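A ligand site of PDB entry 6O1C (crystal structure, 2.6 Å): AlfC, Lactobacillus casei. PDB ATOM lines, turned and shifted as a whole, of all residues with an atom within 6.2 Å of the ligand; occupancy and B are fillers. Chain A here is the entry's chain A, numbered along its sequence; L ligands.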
ATOM      1  N   MET A  16      30.810  23.217 -26.770  1.00  0.00           N
ATOM      2  CA  MET A  16      30.219  22.524 -25.586  1.00  0.00           C
ATOM      3  C   MET A  16      31.255  21.521 -25.096  1.00  0.00           C
ATOM      4  O   MET A  16      32.060  21.074 -25.936  1.00  0.00           O
ATOM      5  CB  MET A  16      28.929  21.810 -25.959  1.00  0.00           C
ATOM      6  CG  MET A  16      28.068  21.428 -24.778  1.00  0.00           C
ATOM      7  SD  MET A  16      26.539  20.611 -25.367  1.00  0.00           S
ATOM      8  CE  MET A  16      25.405  21.159 -24.092  1.00  0.00           C
ATOM      9  N   HIS A  18      31.550  17.990 -22.615  1.00  0.00           N
ATOM     10  CA  HIS A  18      31.150  16.860 -21.751  1.00  0.00           C
ATOM     11  C   HIS A  18      32.413  16.210 -21.199  1.00  0.00           C
ATOM     12  O   HIS A  18      33.288  15.780 -22.023  1.00  0.00           O
ATOM     13  CB  HIS A  18      30.311  15.829 -22.514  1.00  0.00           C
ATOM     14  CG  HIS A  18      28.891  16.212 -22.727  1.00  0.00           C
ATOM     15  ND1 HIS A  18      28.524  17.327 -23.441  1.00  0.00           N
ATOM     16  CD2 HIS A  18      27.756  15.614 -22.341  1.00  0.00           C
ATOM     17  CE1 HIS A  18      27.214  17.407 -23.484  1.00  0.00           C
ATOM     18  NE2 HIS A  18      26.710  16.364 -22.804  1.00  0.00           N
ATOM     19  N   TYR A  37      26.109   6.942 -26.759  1.00  0.00           N
ATOM     20  CA  TYR A  37      26.319   7.929 -25.662  1.00  0.00           C
ATOM     21  C   TYR A  37      27.133   7.257 -24.550  1.00  0.00           C
ATOM     22  O   TYR A  37      26.587   6.521 -23.668  1.00  0.00           O
ATOM     23  CB  TYR A  37      24.986   8.480 -25.155  1.00  0.00           C
ATOM     24  CG  TYR A  37      24.204   9.350 -26.116  1.00  0.00           C
ATOM     25  CD1 TYR A  37      24.622   9.549 -27.418  1.00  0.00           C
ATOM     26  CD2 TYR A  37      23.008   9.939 -25.733  1.00  0.00           C
ATOM     27  CE1 TYR A  37      23.877  10.319 -28.310  1.00  0.00           C
ATOM     28  CE2 TYR A  37      22.267  10.715 -26.604  1.00  0.00           C
ATOM     29  CZ  TYR A  37      22.703  10.903 -27.897  1.00  0.00           C
ATOM     30  OH  TYR A  37      22.034  11.670 -28.798  1.00  0.00           O
ATOM     31  N   GLU A  39      28.719   8.745 -22.154  1.00  0.00           N
ATOM     32  CA  GLU A  39      28.482   9.454 -20.860  1.00  0.00           C
ATOM     33  C   GLU A  39      27.365   8.765 -20.063  1.00  0.00           C
ATOM     34  O   GLU A  39      27.334   8.977 -18.822  1.00  0.00           O
ATOM     35  CB  GLU A  39      28.171  10.936 -21.053  1.00  0.00           C
ATOM     36  CG  GLU A  39      26.865  11.224 -21.782  1.00  0.00           C
ATOM     37  CD  GLU A  39      26.906  11.132 -23.292  1.00  0.00           C
ATOM     38  OE1 GLU A  39      27.993  10.735 -23.862  1.00  0.00           O
ATOM     39  OE2 GLU A  39      25.862  11.454 -23.917  1.00  0.00           O
ATOM     40  N   TRP A  40      26.530   7.948 -20.743  1.00  0.00           N
ATOM     41  CA  TRP A  40      25.412   7.168 -20.147  1.00  0.00           C
ATOM     42  C   TRP A  40      25.893   5.803 -19.653  1.00  0.00           C
ATOM     43  O   TRP A  40      25.035   4.974 -19.311  1.00  0.00           O
ATOM     44  CB  TRP A  40      24.261   6.993 -21.155  1.00  0.00           C
ATOM     45  CG  TRP A  40      23.294   8.140 -21.198  1.00  0.00           C
ATOM     46  CD1 TRP A  40      23.491   9.369 -21.751  1.00  0.00           C
ATOM     47  CD2 TRP A  40      21.967   8.163 -20.654  1.00  0.00           C
ATOM     48  NE1 TRP A  40      22.389  10.152 -21.592  1.00  0.00           N
ATOM     49  CE2 TRP A  40      21.437   9.446 -20.914  1.00  0.00           C
ATOM     50  CE3 TRP A  40      21.179   7.239 -19.960  1.00  0.00           C
ATOM     51  CZ2 TRP A  40      20.149   9.813 -20.507  1.00  0.00           C
ATOM     52  CZ3 TRP A  40      19.907   7.599 -19.568  1.00  0.00           C
ATOM     53  CH2 TRP A  40      19.404   8.872 -19.849  1.00  0.00           C
ATOM     54  N   THR A  84      29.612  20.896 -18.866  1.00  0.00           N
ATOM     55  CA  THR A  84      28.918  20.046 -17.871  1.00  0.00           C
ATOM     56  C   THR A  84      29.429  20.398 -16.463  1.00  0.00           C
ATOM     57  O   THR A  84      30.587  20.072 -16.186  1.00  0.00           O
ATOM     58  CB  THR A  84      29.112  18.558 -18.186  1.00  0.00           C
ATOM     59  OG1 THR A  84      30.512  18.288 -18.282  1.00  0.00           O
ATOM     60  CG2 THR A  84      28.432  18.141 -19.471  1.00  0.00           C
ATOM     61  N   HIS A  87      26.503  16.138 -14.770  1.00  0.00           N
ATOM     62  CA  HIS A  87      25.717  15.351 -15.753  1.00  0.00           C
ATOM     63  C   HIS A  87      24.824  14.394 -14.971  1.00  0.00           C
ATOM     64  O   HIS A  87      24.700  14.597 -13.768  1.00  0.00           O
ATOM     65  CB  HIS A  87      26.651  14.678 -16.763  1.00  0.00           C
ATOM     66  CG  HIS A  87      25.976  14.298 -18.025  1.00  0.00           C
ATOM     67  ND1 HIS A  87      25.540  13.019 -18.257  1.00  0.00           N
ATOM     68  CD2 HIS A  87      25.588  15.054 -19.076  1.00  0.00           C
ATOM     69  CE1 HIS A  87      24.912  12.986 -19.424  1.00  0.00           C
ATOM     70  NE2 HIS A  87      24.931  14.219 -19.947  1.00  0.00           N
ATOM     71  N   HIS A  88      24.225  13.393 -15.625  1.00  0.00           N
ATOM     72  CA  HIS A  88      23.238  12.456 -15.033  1.00  0.00           C
ATOM     73  C   HIS A  88      23.870  11.625 -13.902  1.00  0.00           C
ATOM     74  O   HIS A  88      23.112  11.155 -13.044  1.00  0.00           O
ATOM     75  CB  HIS A  88      22.629  11.560 -16.122  1.00  0.00           C
ATOM     76  CG  HIS A  88      21.985  12.305 -17.261  1.00  0.00           C
ATOM     77  ND1 HIS A  88      21.375  13.547 -17.092  1.00  0.00           N
ATOM     78  CD2 HIS A  88      21.842  11.963 -18.567  1.00  0.00           C
ATOM     79  CE1 HIS A  88      20.892  13.936 -18.257  1.00  0.00           C
ATOM     80  NE2 HIS A  88      21.173  12.983 -19.178  1.00  0.00           N
ATOM     81  N   TYR A 131      25.920  23.824 -18.003  1.00  0.00           N
ATOM     82  CA  TYR A 131      24.971  22.693 -18.160  1.00  0.00           C
ATOM     83  C   TYR A 131      24.836  22.033 -16.788  1.00  0.00           C
ATOM     84  O   TYR A 131      25.857  21.661 -16.197  1.00  0.00           O
ATOM     85  CB  TYR A 131      25.494  21.744 -19.238  1.00  0.00           C
ATOM     86  CG  TYR A 131      24.692  20.486 -19.504  1.00  0.00           C
ATOM     87  CD1 TYR A 131      24.484  19.529 -18.529  1.00  0.00           C
ATOM     88  CD2 TYR A 131      24.202  20.225 -20.771  1.00  0.00           C
ATOM     89  CE1 TYR A 131      23.745  18.383 -18.780  1.00  0.00           C
ATOM     90  CE2 TYR A 131      23.485  19.075 -21.058  1.00  0.00           C
ATOM     91  CZ  TYR A 131      23.249  18.141 -20.055  1.00  0.00           C
ATOM     92  OH  TYR A 131      22.538  17.016 -20.327  1.00  0.00           O
ATOM     93  N   LEU A 136      17.728  14.149 -13.529  1.00  0.00           N
ATOM     94  CA  LEU A 136      18.402  12.841 -13.358  1.00  0.00           C
ATOM     95  C   LEU A 136      19.607  13.053 -12.444  1.00  0.00           C
ATOM     96  O   LEU A 136      20.327  14.052 -12.667  1.00  0.00           O
ATOM     97  CB  LEU A 136      18.849  12.312 -14.723  1.00  0.00           C
ATOM     98  CG  LEU A 136      17.747  12.025 -15.733  1.00  0.00           C
ATOM     99  CD1 LEU A 136      18.286  11.203 -16.904  1.00  0.00           C
ATOM    100  CD2 LEU A 136      16.579  11.302 -15.073  1.00  0.00           C
ATOM    101  N   TRP A 158      16.189   5.523 -16.738  1.00  0.00           N
ATOM    102  CA  TRP A 158      16.434   6.988 -16.575  1.00  0.00           C
ATOM    103  C   TRP A 158      17.045   7.254 -15.195  1.00  0.00           C
ATOM    104  O   TRP A 158      17.943   8.107 -15.113  1.00  0.00           O
ATOM    105  CB  TRP A 158      15.128   7.773 -16.756  1.00  0.00           C
ATOM    106  CG  TRP A 158      14.537   7.737 -18.131  1.00  0.00           C
ATOM    107  CD1 TRP A 158      13.549   6.896 -18.575  1.00  0.00           C
ATOM    108  CD2 TRP A 158      14.848   8.598 -19.240  1.00  0.00           C
ATOM    109  NE1 TRP A 158      13.253   7.154 -19.880  1.00  0.00           N
ATOM    110  CE2 TRP A 158      14.027   8.197 -20.321  1.00  0.00           C
ATOM    111  CE3 TRP A 158      15.748   9.656 -19.426  1.00  0.00           C
ATOM    112  CZ2 TRP A 158      14.076   8.823 -21.565  1.00  0.00           C
ATOM    113  CZ3 TRP A 158      15.781  10.279 -20.652  1.00  0.00           C
ATOM    114  CH2 TRP A 158      14.972   9.852 -21.709  1.00  0.00           C
ATOM    115  N   TRP A 198      21.924  25.938 -19.305  1.00  0.00           N
ATOM    116  CA  TRP A 198      21.557  24.799 -20.169  1.00  0.00           C
ATOM    117  C   TRP A 198      21.046  23.658 -19.292  1.00  0.00           C
ATOM    118  O   TRP A 198      21.898  22.990 -18.644  1.00  0.00           O
ATOM    119  CB  TRP A 198      22.785  24.364 -20.979  1.00  0.00           C
ATOM    120  CG  TRP A 198      22.569  24.246 -22.451  1.00  0.00           C
ATOM    121  CD1 TRP A 198      22.782  25.196 -23.411  1.00  0.00           C
ATOM    122  CD2 TRP A 198      22.182  23.048 -23.136  1.00  0.00           C
ATOM    123  NE1 TRP A 198      22.520  24.672 -24.638  1.00  0.00           N
ATOM    124  CE2 TRP A 198      22.155  23.351 -24.514  1.00  0.00           C
ATOM    125  CE3 TRP A 198      21.828  21.758 -22.721  1.00  0.00           C
ATOM    126  CZ2 TRP A 198      21.785  22.417 -25.470  1.00  0.00           C
ATOM    127  CZ3 TRP A 198      21.465  20.827 -23.665  1.00  0.00           C
ATOM    128  CH2 TRP A 198      21.451  21.157 -25.016  1.00  0.00           C
ATOM    129  N   VAL A 201      16.362  17.593 -20.152  1.00  0.00           N
ATOM    130  CA  VAL A 201      14.917  17.357 -20.438  1.00  0.00           C
ATOM    131  C   VAL A 201      14.274  16.920 -19.126  1.00  0.00           C
ATOM    132  O   VAL A 201      14.681  15.926 -18.517  1.00  0.00           O
ATOM    133  CB  VAL A 201      14.739  16.322 -21.575  1.00  0.00           C
ATOM    134  CG1 VAL A 201      15.038  16.919 -22.940  1.00  0.00           C
ATOM    135  CG2 VAL A 201      15.641  15.092 -21.348  1.00  0.00           C
ATOM    136  N   ARG A 229      14.710  23.899 -22.480  1.00  0.00           N
ATOM    137  CA  ARG A 229      14.600  22.563 -21.853  1.00  0.00           C
ATOM    138  C   ARG A 229      14.290  22.647 -20.359  1.00  0.00           C
ATOM    139  O   ARG A 229      14.211  21.582 -19.725  1.00  0.00           O
ATOM    140  CB  ARG A 229      15.892  21.764 -22.045  1.00  0.00           C
ATOM    141  CG  ARG A 229      16.107  21.283 -23.467  1.00  0.00           C
ATOM    142  CD  ARG A 229      17.017  20.051 -23.457  1.00  0.00           C
ATOM    143  NE  ARG A 229      16.810  19.364 -24.711  1.00  0.00           N
ATOM    144  CZ  ARG A 229      17.414  19.676 -25.861  1.00  0.00           C
ATOM    145  NH1 ARG A 229      18.320  20.645 -25.882  1.00  0.00           N
ATOM    146  NH2 ARG A 229      17.117  19.025 -26.967  1.00  0.00           N
ATOM    147  N   LEU A 240      16.741  23.577 -30.272  1.00  0.00           N
ATOM    148  CA  LEU A 240      16.148  22.750 -31.368  1.00  0.00           C
ATOM    149  C   LEU A 240      16.853  21.400 -31.393  1.00  0.00           C
ATOM    150  O   LEU A 240      18.093  21.429 -31.409  1.00  0.00           O
ATOM    151  CB  LEU A 240      16.295  23.473 -32.702  1.00  0.00           C
ATOM    152  CG  LEU A 240      15.526  24.793 -32.808  1.00  0.00           C
ATOM    153  CD1 LEU A 240      16.066  25.698 -33.904  1.00  0.00           C
ATOM    154  CD2 LEU A 240      14.043  24.522 -32.984  1.00  0.00           C
ATOM    155  N   GLY A 241      16.056  20.313 -31.363  1.00  0.00           N
ATOM    156  CA  GLY A 241      16.514  18.936 -31.600  1.00  0.00           C
ATOM    157  C   GLY A 241      16.751  18.741 -33.079  1.00  0.00           C
ATOM    158  O   GLY A 241      16.161  19.508 -33.867  1.00  0.00           O
ATOM    159  N   ASP A 242      17.591  17.760 -33.463  1.00  0.00           N
ATOM    160  CA  ASP A 242      17.999  17.557 -34.885  1.00  0.00           C
ATOM    161  C   ASP A 242      16.763  17.491 -35.781  1.00  0.00           C
ATOM    162  O   ASP A 242      16.776  18.122 -36.850  1.00  0.00           O
ATOM    163  CB  ASP A 242      18.894  16.339 -35.050  1.00  0.00           C
ATOM    164  CG  ASP A 242      20.279  16.625 -34.480  1.00  0.00           C
ATOM    165  OD1 ASP A 242      20.939  17.593 -34.942  1.00  0.00           O
ATOM    166  OD2 ASP A 242      20.691  15.898 -33.531  1.00  0.00           O
ATOM    167  N   ASN A 243      15.742  16.777 -35.309  1.00  0.00           N
ATOM    168  CA  ASN A 243      14.433  16.570 -36.003  1.00  0.00           C
ATOM    169  C   ASN A 243      13.649  17.889 -36.157  1.00  0.00           C
ATOM    170  O   ASN A 243      12.532  17.810 -36.681  1.00  0.00           O
ATOM    171  CB  ASN A 243      13.575  15.561 -35.236  1.00  0.00           C
ATOM    172  CG  ASN A 243      13.240  16.053 -33.834  1.00  0.00           C
ATOM    173  OD1 ASN A 243      14.138  16.407 -33.055  1.00  0.00           O
ATOM    174  ND2 ASN A 243      11.958  16.109 -33.518  1.00  0.00           N
ATOM    175  N   THR A 275      21.014  24.922 -31.885  1.00  0.00           N
ATOM    176  CA  THR A 275      21.067  23.450 -31.964  1.00  0.00           C
ATOM    177  C   THR A 275      22.447  22.984 -31.482  1.00  0.00           C
ATOM    178  O   THR A 275      23.471  23.562 -31.918  1.00  0.00           O
ATOM    179  CB  THR A 275      20.722  22.911 -33.355  1.00  0.00           C
ATOM    180  OG1 THR A 275      20.462  21.526 -33.110  1.00  0.00           O
ATOM    181  CG2 THR A 275      21.785  22.991 -34.425  1.00  0.00           C
ATOM    182  N   ALA A 276      22.459  22.020 -30.567  1.00  0.00           N
ATOM    183  CA  ALA A 276      23.660  21.349 -30.050  1.00  0.00           C
ATOM    184  C   ALA A 276      23.926  20.113 -30.902  1.00  0.00           C
ATOM    185  O   ALA A 276      22.971  19.403 -31.204  1.00  0.00           O
ATOM    186  CB  ALA A 276      23.481  20.979 -28.603  1.00  0.00           C
ATOM    187  N   TRP A 283      28.670  12.229 -26.822  1.00  0.00           N
ATOM    188  CA  TRP A 283      28.915  13.531 -26.140  1.00  0.00           C
ATOM    189  C   TRP A 283      30.159  13.356 -25.271  1.00  0.00           C
ATOM    190  O   TRP A 283      31.121  14.129 -25.395  1.00  0.00           O
ATOM    191  CB  TRP A 283      27.662  13.965 -25.381  1.00  0.00           C
ATOM    192  CG  TRP A 283      26.478  14.134 -26.274  1.00  0.00           C
ATOM    193  CD1 TRP A 283      25.539  13.196 -26.593  1.00  0.00           C
ATOM    194  CD2 TRP A 283      26.094  15.326 -26.987  1.00  0.00           C
ATOM    195  NE1 TRP A 283      24.612  13.719 -27.447  1.00  0.00           N
ATOM    196  CE2 TRP A 283      24.926  15.029 -27.705  1.00  0.00           C
ATOM    197  CE3 TRP A 283      26.623  16.615 -27.070  1.00  0.00           C
ATOM    198  CZ2 TRP A 283      24.271  15.974 -28.496  1.00  0.00           C
ATOM    199  CZ3 TRP A 283      25.986  17.549 -27.852  1.00  0.00           C
ATOM    200  CH2 TRP A 283      24.820  17.226 -28.550  1.00  0.00           C
HETATM  201  C1  LIG L   1      20.891  14.580 -23.434  1.00  0.00           C
HETATM  202  C2  LIG L   1      21.791  13.821 -22.464  1.00  0.00           C
HETATM  203  O1  LIG L   1      21.105  12.652 -22.051  1.00  0.00           O
HETATM  204  C3  LIG L   1      23.151  13.491 -23.213  1.00  0.00           C
HETATM  205  O2  LIG L   1      23.986  12.650 -22.411  1.00  0.00           O
HETATM  206  C4  LIG L   1      23.843  14.871 -23.585  1.00  0.00           C
HETATM  207  O3  LIG L   1      24.087  15.607 -22.468  1.00  0.00           O
HETATM  208  C5  LIG L   1      22.898  15.672 -24.540  1.00  0.00           C
HETATM  209  C6  LIG L   1      23.542  17.083 -24.761  1.00  0.00           C
HETATM  210  O4  LIG L   1      21.553  15.729 -24.034  1.00  0.00           O
HETATM  211  O5  LIG L   1      20.296  13.652 -24.408  1.00  0.00           O
HETATM  212  C7  LIG L   1      19.833  14.377 -25.494  1.00  0.00           C
HETATM  213  C8  LIG L   1      20.622  14.404 -26.699  1.00  0.00           C
HETATM  214  C9  LIG L   1      20.240  15.169 -27.828  1.00  0.00           C
HETATM  215  C10 LIG L   1      19.065  15.931 -27.773  1.00  0.00           C
HETATM  216  C11 LIG L   1      18.250  15.969 -26.576  1.00  0.00           C
HETATM  217  C12 LIG L   1      18.641  15.195 -25.441  1.00  0.00           C
HETATM  218  N1  LIG L   1      18.817  16.730 -29.113  1.00  0.00           N
HETATM  219  O6  LIG L   1      19.625  17.446 -29.576  1.00  0.00           O
HETATM  220  O7  LIG L   1      17.696  16.488 -29.549  1.00  0.00           O
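OE2 of Glu 39 lies within hydrogen-bond range of O2 of the ligand (2.7 Å). O3 of the ligand is in hydrogen-bond range of NE2 of His 18 (2.8 Å). The indole nitrogen (NE1) of Trp 40 lies within hydrogen-bond range of an oxygen (O1) of the ligand (2.8 Å). An oxygen (O1) of the ligand is in hydrogen-bond range of a ring nitrogen (NE2) of His 88 (2.9 Å). OH of Tyr 131 sits at hydrogen-bond distance from O3 of the ligand (3.0 Å). A ring nitrogen (NE2) of His 87 lies within hydrogen-bond range of an oxygen (O3) of the ligand, at 3.0 Å.
Tyr 37 touches the ligand (OH to C8, 3.7 Å). Arg 229 touches the ligand. CA of Gly 241 touches O7 of the ligand, at 3.4 Å. Trp 283 touches the ligand (CE2 to C5, 3.8 Å). Along chain A the residues within 4 Å of the ligand span positions 18 to 283. The nearest printed residue that does not touch the ligand is Asp 242 (4.1 Å).
OE1 of Glu 39 is in hydrogen-bond range of N of Trp 283 (3.4 Å).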
